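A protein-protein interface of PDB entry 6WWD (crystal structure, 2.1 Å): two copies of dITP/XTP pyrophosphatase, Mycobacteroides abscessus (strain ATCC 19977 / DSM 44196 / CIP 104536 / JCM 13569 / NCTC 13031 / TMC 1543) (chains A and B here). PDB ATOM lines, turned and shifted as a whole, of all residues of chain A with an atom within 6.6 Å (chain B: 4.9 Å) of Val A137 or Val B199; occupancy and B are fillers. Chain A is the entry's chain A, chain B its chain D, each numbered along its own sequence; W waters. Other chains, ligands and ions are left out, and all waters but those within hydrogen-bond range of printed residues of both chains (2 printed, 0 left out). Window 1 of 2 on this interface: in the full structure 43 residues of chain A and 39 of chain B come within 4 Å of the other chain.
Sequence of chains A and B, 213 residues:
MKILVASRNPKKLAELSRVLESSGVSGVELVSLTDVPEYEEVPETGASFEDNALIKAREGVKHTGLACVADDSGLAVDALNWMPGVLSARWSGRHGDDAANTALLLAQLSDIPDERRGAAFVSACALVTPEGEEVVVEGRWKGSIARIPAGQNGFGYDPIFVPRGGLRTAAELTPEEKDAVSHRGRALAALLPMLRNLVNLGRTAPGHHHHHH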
ATOM      1  N   GLU A  50      16.518  33.050  13.909  1.00  0.00           N
ATOM      2  CA  GLU A  50      17.272  33.001  15.159  1.00  0.00           C
ATOM      3  C   GLU A  50      17.809  34.375  15.538  1.00  0.00           C
ATOM      4  O   GLU A  50      17.668  34.800  16.688  1.00  0.00           O
ATOM      5  CB  GLU A  50      18.424  31.996  15.058  1.00  0.00           C
ATOM      6  CG  GLU A  50      17.963  30.542  14.991  1.00  0.00           C
ATOM      7  CD  GLU A  50      19.131  29.553  15.061  1.00  0.00           C
ATOM      8  OE1 GLU A  50      20.291  30.016  15.136  1.00  0.00           O
ATOM      9  OE2 GLU A  50      18.883  28.322  15.064  1.00  0.00           O
ATOM     10  N   ALA A  53      14.878  36.687  16.570  1.00  0.00           N
ATOM     11  CA  ALA A  53      14.362  36.362  17.897  1.00  0.00           C
ATOM     12  C   ALA A  53      15.296  36.868  19.000  1.00  0.00           C
ATOM     13  O   ALA A  53      14.831  37.392  20.019  1.00  0.00           O
ATOM     14  CB  ALA A  53      14.119  34.857  18.009  1.00  0.00           C
ATOM     15  N   SER A 123      10.570  27.890  13.044  1.00  0.00           N
ATOM     16  CA  SER A 123      10.067  28.536  14.250  1.00  0.00           C
ATOM     17  C   SER A 123      11.244  28.645  15.213  1.00  0.00           C
ATOM     18  O   SER A 123      11.748  27.622  15.692  1.00  0.00           O
ATOM     19  CB  SER A 123       8.928  27.709  14.850  1.00  0.00           C
ATOM     20  OG  SER A 123       8.464  28.258  16.048  1.00  0.00           O
ATOM     21  N   ALA A 124      11.672  29.874  15.509  1.00  0.00           N
ATOM     22  CA  ALA A 124      12.804  30.115  16.390  1.00  0.00           C
ATOM     23  C   ALA A 124      12.342  30.830  17.654  1.00  0.00           C
ATOM     24  O   ALA A 124      11.371  31.586  17.627  1.00  0.00           O
ATOM     25  CB  ALA A 124      13.883  30.943  15.691  1.00  0.00           C
ATOM     26  N   CYS A 125      13.066  30.590  18.753  1.00  0.00           N
ATOM     27  CA  CYS A 125      12.756  31.129  20.076  1.00  0.00           C
ATOM     28  C   CYS A 125      14.054  31.489  20.776  1.00  0.00           C
ATOM     29  O   CYS A 125      14.989  30.684  20.780  1.00  0.00           O
ATOM     30  CB  CYS A 125      12.010  30.115  20.940  1.00  0.00           C
ATOM     31  SG  CYS A 125      10.534  29.478  20.209  1.00  0.00           S
ATOM     32  N   ALA A 126      14.108  32.675  21.396  1.00  0.00           N
ATOM     33  CA  ALA A 126      15.318  33.108  22.084  1.00  0.00           C
ATOM     34  C   ALA A 126      15.035  33.439  23.540  1.00  0.00           C
ATOM     35  O   ALA A 126      13.942  33.886  23.898  1.00  0.00           O
ATOM     36  CB  ALA A 126      15.972  34.324  21.429  1.00  0.00           C
ATOM     37  N   LEU A 127      16.050  33.210  24.365  1.00  0.00           N
ATOM     38  CA  LEU A 127      16.071  33.598  25.764  1.00  0.00           C
ATOM     39  C   LEU A 127      17.292  34.482  26.019  1.00  0.00           C
ATOM     40  O   LEU A 127      18.400  34.147  25.581  1.00  0.00           O
ATOM     41  CB  LEU A 127      16.147  32.357  26.632  1.00  0.00           C
ATOM     42  CG  LEU A 127      16.530  32.661  28.058  1.00  0.00           C
ATOM     43  CD1 LEU A 127      15.312  33.252  28.717  1.00  0.00           C
ATOM     44  CD2 LEU A 127      17.066  31.405  28.747  1.00  0.00           C
ATOM     45  N   VAL A 135      20.603  32.257  24.684  1.00  0.00           N
ATOM     46  CA  VAL A 135      20.346  30.955  24.087  1.00  0.00           C
ATOM     47  C   VAL A 135      19.243  31.138  23.059  1.00  0.00           C
ATOM     48  O   VAL A 135      18.240  31.810  23.324  1.00  0.00           O
ATOM     49  CB  VAL A 135      19.918  29.903  25.133  1.00  0.00           C
ATOM     50  CG1 VAL A 135      19.638  28.559  24.451  1.00  0.00           C
ATOM     51  CG2 VAL A 135      20.987  29.737  26.206  1.00  0.00           C
ATOM     52  N   VAL A 136      19.416  30.550  21.888  1.00  0.00           N
ATOM     53  CA  VAL A 136      18.371  30.576  20.879  1.00  0.00           C
ATOM     54  C   VAL A 136      18.201  29.158  20.350  1.00  0.00           C
ATOM     55  O   VAL A 136      19.182  28.423  20.181  1.00  0.00           O
ATOM     56  CB  VAL A 136      18.683  31.581  19.745  1.00  0.00           C
ATOM     57  CG1 VAL A 136      19.928  31.171  18.969  1.00  0.00           C
ATOM     58  CG2 VAL A 136      17.485  31.743  18.817  1.00  0.00           C
ATOM     59  N   VAL A 137      16.953  28.759  20.144  1.00  0.00           N
ATOM     60  CA  VAL A 137      16.622  27.490  19.517  1.00  0.00           C
ATOM     61  C   VAL A 137      15.775  27.762  18.277  1.00  0.00           C
ATOM     62  O   VAL A 137      15.104  28.793  18.162  1.00  0.00           O
ATOM     63  CB  VAL A 137      15.890  26.539  20.483  1.00  0.00           C
ATOM     64  CG1 VAL A 137      16.671  26.401  21.790  1.00  0.00           C
ATOM     65  CG2 VAL A 137      14.484  27.012  20.753  1.00  0.00           C
ATOM     66  N   GLU A 138      15.829  26.827  17.326  1.00  0.00           N
ATOM     67  CA  GLU A 138      14.908  26.851  16.199  1.00  0.00           C
ATOM     68  C   GLU A 138      14.522  25.424  15.847  1.00  0.00           C
ATOM     69  O   GLU A 138      15.283  24.484  16.091  1.00  0.00           O
ATOM     70  CB  GLU A 138      15.520  27.561  14.969  1.00  0.00           C
ATOM     71  CG  GLU A 138      16.398  26.653  14.099  1.00  0.00           C
ATOM     72  CD  GLU A 138      16.854  27.311  12.814  1.00  0.00           C
ATOM     73  OE1 GLU A 138      16.435  28.464  12.519  1.00  0.00           O
ATOM     74  OE2 GLU A 138      17.640  26.666  12.087  1.00  0.00           O
ATOM     75  N   GLY A 139      13.328  25.271  15.297  1.00  0.00           N
ATOM     76  CA  GLY A 139      12.907  24.019  14.684  1.00  0.00           C
ATOM     77  C   GLY A 139      12.554  24.280  13.232  1.00  0.00           C
ATOM     78  O   GLY A 139      12.047  25.360  12.902  1.00  0.00           O
ATOM     79  N   ARG A 140      12.861  23.305  12.360  1.00  0.00           N
ATOM     80  CA  ARG A 140      12.570  23.376  10.928  1.00  0.00           C
ATOM     81  C   ARG A 140      11.791  22.143  10.515  1.00  0.00           C
ATOM     82  O   ARG A 140      12.240  21.016  10.752  1.00  0.00           O
ATOM     83  CB  ARG A 140      13.837  23.459  10.072  1.00  0.00           C
ATOM     84  CG  ARG A 140      14.619  24.698  10.284  1.00  0.00           C
ATOM     85  CD  ARG A 140      15.738  24.915   9.266  1.00  0.00           C
ATOM     86  NE  ARG A 140      16.330  26.203   9.610  1.00  0.00           N
ATOM     87  CZ  ARG A 140      16.333  27.271   8.825  1.00  0.00           C
ATOM     88  NH1 ARG A 140      15.834  27.196   7.586  1.00  0.00           N
ATOM     89  NH2 ARG A 140      16.865  28.409   9.276  1.00  0.00           N
ATOM     90  N   VAL A 181       3.062  16.951  14.730  1.00  0.00           N
ATOM     91  CA  VAL A 181       4.289  17.565  14.224  1.00  0.00           C
ATOM     92  C   VAL A 181       4.873  18.552  15.239  1.00  0.00           C
ATOM     93  O   VAL A 181       6.097  18.664  15.382  1.00  0.00           O
ATOM     94  CB  VAL A 181       4.009  18.224  12.859  1.00  0.00           C
ATOM     95  CG1 VAL A 181       5.175  19.087  12.411  1.00  0.00           C
ATOM     96  CG2 VAL A 181       3.708  17.152  11.816  1.00  0.00           C
ATOM     97  N   SER A 182       4.019  19.272  15.968  1.00  0.00           N
ATOM     98  CA  SER A 182       4.511  20.113  17.058  1.00  0.00           C
ATOM     99  C   SER A 182       4.982  19.279  18.244  1.00  0.00           C
ATOM    100  O   SER A 182       5.904  19.690  18.957  1.00  0.00           O
ATOM    101  CB  SER A 182       3.430  21.099  17.512  1.00  0.00           C
ATOM    102  OG  SER A 182       3.347  22.215  16.642  1.00  0.00           O
ATOM    103  N   GLY A 185       8.426  18.104  17.274  1.00  0.00           N
ATOM    104  CA  GLY A 185       9.338  19.240  17.304  1.00  0.00           C
ATOM    105  C   GLY A 185       9.731  19.629  18.719  1.00  0.00           C
ATOM    106  O   GLY A 185      10.901  19.883  19.008  1.00  0.00           O
ATOM    107  N   ARG A 186       8.746  19.702  19.616  1.00  0.00           N
ATOM    108  CA  ARG A 186       9.017  20.035  21.011  1.00  0.00           C
ATOM    109  C   ARG A 186       9.760  18.915  21.741  1.00  0.00           C
ATOM    110  O   ARG A 186      10.506  19.191  22.690  1.00  0.00           O
ATOM    111  CB  ARG A 186       7.704  20.382  21.710  1.00  0.00           C
ATOM    112  CG  ARG A 186       7.073  21.641  21.150  1.00  0.00           C
ATOM    113  CD  ARG A 186       5.620  21.789  21.559  1.00  0.00           C
ATOM    114  NE  ARG A 186       5.114  23.111  21.201  1.00  0.00           N
ATOM    115  CZ  ARG A 186       3.828  23.435  21.144  1.00  0.00           C
ATOM    116  NH1 ARG A 186       2.900  22.526  21.409  1.00  0.00           N
ATOM    117  NH2 ARG A 186       3.471  24.669  20.812  1.00  0.00           N
ATOM    118  N   ALA A 189      13.352  19.332  20.698  1.00  0.00           N
ATOM    119  CA  ALA A 189      13.930  20.486  21.373  1.00  0.00           C
ATOM    120  C   ALA A 189      14.333  20.141  22.801  1.00  0.00           C
ATOM    121  O   ALA A 189      15.345  20.645  23.302  1.00  0.00           O
ATOM    122  CB  ALA A 189      12.936  21.648  21.370  1.00  0.00           C
ATOM    123  N   LEU A 192      17.836  18.046  22.821  1.00  0.00           N
ATOM    124  CA  LEU A 192      19.083  18.737  22.472  1.00  0.00           C
ATOM    125  C   LEU A 192      20.140  18.615  23.568  1.00  0.00           C
ATOM    126  O   LEU A 192      19.956  19.129  24.679  1.00  0.00           O
ATOM    127  CB  LEU A 192      18.826  20.222  22.193  1.00  0.00           C
ATOM    128  CG  LEU A 192      18.060  20.588  20.923  1.00  0.00           C
ATOM    129  CD1 LEU A 192      17.960  22.082  20.784  1.00  0.00           C
ATOM    130  CD2 LEU A 192      18.778  20.002  19.729  1.00  0.00           C
ATOM    131  N   MET A 194      23.031  20.106  24.181  1.00  0.00           N
ATOM    132  CA  MET A 194      23.629  21.306  24.769  1.00  0.00           C
ATOM    133  C   MET A 194      22.715  21.940  25.808  1.00  0.00           C
ATOM    134  O   MET A 194      23.202  22.621  26.721  1.00  0.00           O
ATOM    135  CB  MET A 194      23.994  22.316  23.677  1.00  0.00           C
ATOM    136  CG  MET A 194      24.562  23.644  24.158  1.00  0.00           C
ATOM    137  SD  MET A 194      23.275  24.851  24.563  1.00  0.00           S
ATOM    138  CE  MET A 194      22.641  25.256  22.953  1.00  0.00           C
ATOM    139  N   VAL B 137      15.862  20.317  14.833  1.00  0.00           N
ATOM    140  CA  VAL B 137      15.902  21.374  15.834  1.00  0.00           C
ATOM    141  C   VAL B 137      17.364  21.633  16.177  1.00  0.00           C
ATOM    142  O   VAL B 137      18.192  20.721  16.147  1.00  0.00           O
ATOM    143  CB  VAL B 137      15.088  20.993  17.098  1.00  0.00           C
ATOM    144  CG1 VAL B 137      15.137  22.095  18.160  1.00  0.00           C
ATOM    145  CG2 VAL B 137      13.653  20.677  16.738  1.00  0.00           C
ATOM    146  N   GLU B 138      17.686  22.885  16.503  1.00  0.00           N
ATOM    147  CA  GLU B 138      19.016  23.171  17.023  1.00  0.00           C
ATOM    148  C   GLU B 138      18.908  24.165  18.169  1.00  0.00           C
ATOM    149  O   GLU B 138      17.933  24.924  18.273  1.00  0.00           O
ATOM    150  CB  GLU B 138      19.973  23.699  15.943  1.00  0.00           C
ATOM    151  CG  GLU B 138      19.885  25.191  15.714  1.00  0.00           C
ATOM    152  CD  GLU B 138      20.942  25.695  14.743  1.00  0.00           C
ATOM    153  OE1 GLU B 138      20.910  26.910  14.413  1.00  0.00           O
ATOM    154  OE2 GLU B 138      21.792  24.872  14.306  1.00  0.00           O
ATOM    155  N   GLY B 139      19.890  24.101  19.057  1.00  0.00           N
ATOM    156  CA  GLY B 139      20.080  25.102  20.091  1.00  0.00           C
ATOM    157  C   GLY B 139      21.466  25.703  19.966  1.00  0.00           C
ATOM    158  O   GLY B 139      22.426  24.995  19.651  1.00  0.00           O
ATOM    159  N   LEU B 195      11.578  27.817  25.804  1.00  0.00           N
ATOM    160  CA  LEU B 195      12.118  27.736  24.449  1.00  0.00           C
ATOM    161  C   LEU B 195      11.639  26.473  23.739  1.00  0.00           C
ATOM    162  O   LEU B 195      11.391  26.498  22.527  1.00  0.00           O
ATOM    163  CB  LEU B 195      13.650  27.791  24.476  1.00  0.00           C
ATOM    164  CG  LEU B 195      14.298  29.086  24.977  1.00  0.00           C
ATOM    165  CD1 LEU B 195      15.653  29.290  24.358  1.00  0.00           C
ATOM    166  CD2 LEU B 195      13.416  30.300  24.731  1.00  0.00           C
ATOM    167  N   ARG B 196      11.473  25.373  24.478  1.00  0.00           N
ATOM    168  CA  ARG B 196      11.040  24.123  23.860  1.00  0.00           C
ATOM    169  C   ARG B 196       9.610  24.228  23.338  1.00  0.00           C
ATOM    170  O   ARG B 196       9.339  23.882  22.181  1.00  0.00           O
ATOM    171  CB  ARG B 196      11.179  22.972  24.858  1.00  0.00           C
ATOM    172  N   ASN B 197       8.681  24.716  24.166  1.00  0.00           N
ATOM    173  CA  ASN B 197       7.280  24.764  23.750  1.00  0.00           C
ATOM    174  C   ASN B 197       7.070  25.715  22.580  1.00  0.00           C
ATOM    175  O   ASN B 197       6.291  25.424  21.663  1.00  0.00           O
ATOM    176  CB  ASN B 197       6.387  25.178  24.918  1.00  0.00           C
ATOM    177  CG  ASN B 197       4.892  25.056  24.594  1.00  0.00           C
ATOM    178  OD1 ASN B 197       4.307  23.977  24.698  1.00  0.00           O
ATOM    179  ND2 ASN B 197       4.275  26.170  24.214  1.00  0.00           N
ATOM    180  N   LEU B 198       7.747  26.861  22.590  1.00  0.00           N
ATOM    181  CA  LEU B 198       7.429  27.875  21.595  1.00  0.00           C
ATOM    182  C   LEU B 198       7.942  27.508  20.200  1.00  0.00           C
ATOM    183  O   LEU B 198       7.491  28.107  19.218  1.00  0.00           O
ATOM    184  CB  LEU B 198       7.954  29.234  22.064  1.00  0.00           C
ATOM    185  N   VAL B 199       8.853  26.536  20.085  1.00  0.00           N
ATOM    186  CA  VAL B 199       9.132  25.901  18.796  1.00  0.00           C
ATOM    187  C   VAL B 199       7.863  25.154  18.392  1.00  0.00           C
ATOM    188  O   VAL B 199       7.614  24.029  18.846  1.00  0.00           O
ATOM    189  CB  VAL B 199      10.360  24.968  18.864  1.00  0.00           C
ATOM    190  CG1 VAL B 199      10.457  24.076  17.636  1.00  0.00           C
ATOM    191  CG2 VAL B 199      11.631  25.776  18.987  1.00  0.00           C
ATOM    192  N   ASN B 200       7.032  25.790  17.567  1.00  0.00           N
ATOM    193  CA  ASN B 200       5.696  25.291  17.245  1.00  0.00           C
ATOM    194  C   ASN B 200       5.568  25.142  15.726  1.00  0.00           C
ATOM    195  O   ASN B 200       5.016  26.008  15.041  1.00  0.00           O
ATOM    196  CB  ASN B 200       4.660  26.223  17.818  1.00  0.00           C
ATOM    197  CG  ASN B 200       3.270  25.668  17.717  1.00  0.00           C
ATOM    198  OD1 ASN B 200       3.067  24.556  17.228  1.00  0.00           O
ATOM    199  ND2 ASN B 200       2.295  26.431  18.196  1.00  0.00           N
ATOM    200  N   LEU B 201       6.046  24.008  15.210  1.00  0.00           N
ATOM    201  CA  LEU B 201       6.198  23.830  13.768  1.00  0.00           C
ATOM    202  C   LEU B 201       4.862  23.566  13.083  1.00  0.00           C
ATOM    203  O   LEU B 201       4.520  24.241  12.103  1.00  0.00           O
ATOM    204  CB  LEU B 201       7.172  22.689  13.489  1.00  0.00           C
ATOM    205  CG  LEU B 201       8.582  23.046  13.927  1.00  0.00           C
ATOM    206  CD1 LEU B 201       9.417  21.807  14.021  1.00  0.00           C
ATOM    207  CD2 LEU B 201       9.164  24.022  12.930  1.00  0.00           C
HETATM  208  O   HOH W   1       7.574  21.828  17.270  1.00  0.00           O
HETATM  209  O   HOH W   2      20.135  27.500  11.311  1.00  0.00           O
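O of Ser A123 lies within hydrogen-bond range of N of Gly A139 (2.9 Å).
The backbone NH (N) of Cys A125 lies within hydrogen-bond range of the backbone carbonyl oxygen (O) of Val A137.
The backbone NH of Leu A127 sits at hydrogen-bond distance from the backbone carbonyl oxygen of Val A135 (2.8 Å).
OE2 of Glu A138 is in salt-bridge range of NE of Arg A140.
Val A137 touches Glu B138, and with the chains exchanged Glu A138 touches Val B137.
Glu B138 touches its own counterpart, Glu A138.
Gly A139 touches Val B137, but with the chains exchanged Val A137 does not touch Gly B139 (4.02 Å).
3 positions are printed for both chains.
Of the 33 pairs that touch across the chains among the printed residues, 3 have their exchanged pair printed and touching as well.
Water W1 lies within hydrogen-bond range of the backbone carbonyl oxygen of Val B199 (2.7 Å), the backbone carbonyl oxygen of Ser A182 (3.2 Å), the backbone NH of Leu B201 (3.4 Å) and the backbone NH of Arg A186 (3.4 Å).
Water W2 lies within hydrogen-bond range of the side-chain carboxylate of Glu A138 and the side-chain carboxylate of Glu B138.
Ala A124 touches none of the printed residues of chain B.
Of the printed residues of chain B, Val A135 touches Leu B195 (3.8 Å).
Of the printed residues of chain B, Val A137 touches Glu B138 (3.1 Å), Leu B195 (3.6 Å) and Val B199 (3.6 Å).
Of the printed residues of chain A, Asn B197 touches Arg A186.
Printed residues of chain A within 4 Å of Leu B198: Ser A123 (3.3 Å) and Cys A125 (3.2 Å).
Of the printed residues of chain A, Val B199 touches Ser A123 (3.7 Å), Cys A125 (3.4 Å), Val A137 (3.6 Å), Gly A139 (3.8 Å) and Arg A186 (3.4 Å).
Printed residues of chain A within 4 Å of Leu B201: Gly A139, Arg A140 and Ser A182.
The nearest residue of chain B that does not touch Val A137 is Gly B139 (4.02 Å).
Printed residues of chain A that touch a printed residue of chain B: Glu A50, Ser A123, Cys A125, Ala A126, Leu A127, Val A135, Val A136, Val A137, Glu A138, Gly A139, Arg A140, Ser A182, Gly A185, Arg A186, Ala A189, Leu A192 and Met A194.
Hydrophobic or aromatic side chains of chain A that line the printed part of chain B: Leu A127, Val A137, Ala A189, Leu A192 and Met A194.
Among the printed residues, no Asp or Glu carboxylate lies within 4 Å of a Lys or Arg side-chain nitrogen of the other chain.
Leu B195 touches Cys A125 (O to SG, 3.9 Å).
CB of Leu A127 touches CD1 of Leu B195, 3.8 Å away.
CA of Val A137 touches O of Glu B138 (3.1 Å).
Val A137 touches Leu B195 (CG2 to O, 3.6 Å).
O of Glu A138 touches CG1 of Val B137 (3.2 Å).
Leu B201 touches Ser A182 (N to OG, 3.5 Å).
O of Gly A185 touches CG2 of Val B137 (3.7 Å).
Arg A186 touches Arg B196.
Val B137 touches Leu A192.
Leu A192 touches Gly B139.
The side-chain carboxylate (OE2) of Glu A50 sits close to the side-chain carboxylate (OE1) of Glu B138.
OG of Ser A123 lies within hydrogen-bond range of O of Leu B198 (3.3 Å).
OG of Ser A123 is in hydrogen-bond range of N of Asn B200, 3.2 Å away.
The side-chain sulfur (SG) of Cys A125 sits close to the backbone carbonyl oxygen (O) of Leu B198 (3.5 Å).
The side-chain sulfur of Cys A125 is in hydrogen-bond range of the backbone NH of Val B199, at 3.4 Å.
The backbone NH (N) of Glu B138 lies within hydrogen-bond range of the backbone carbonyl oxygen (O) of Glu A138, at 2.9 Å.
The side-chain hydroxyl of Ser A182 sits at hydrogen-bond distance from the side-chain amide oxygen of Asn B200.
The backbone carbonyl oxygen of Asn B197 lies within hydrogen-bond range of the guanidinium group of Arg A186 (2.6 Å).
The guanidinium group (NH2) of Arg A186 lies close to the side-chain amide nitrogen (ND2) of Asn B200 (3.4 Å).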
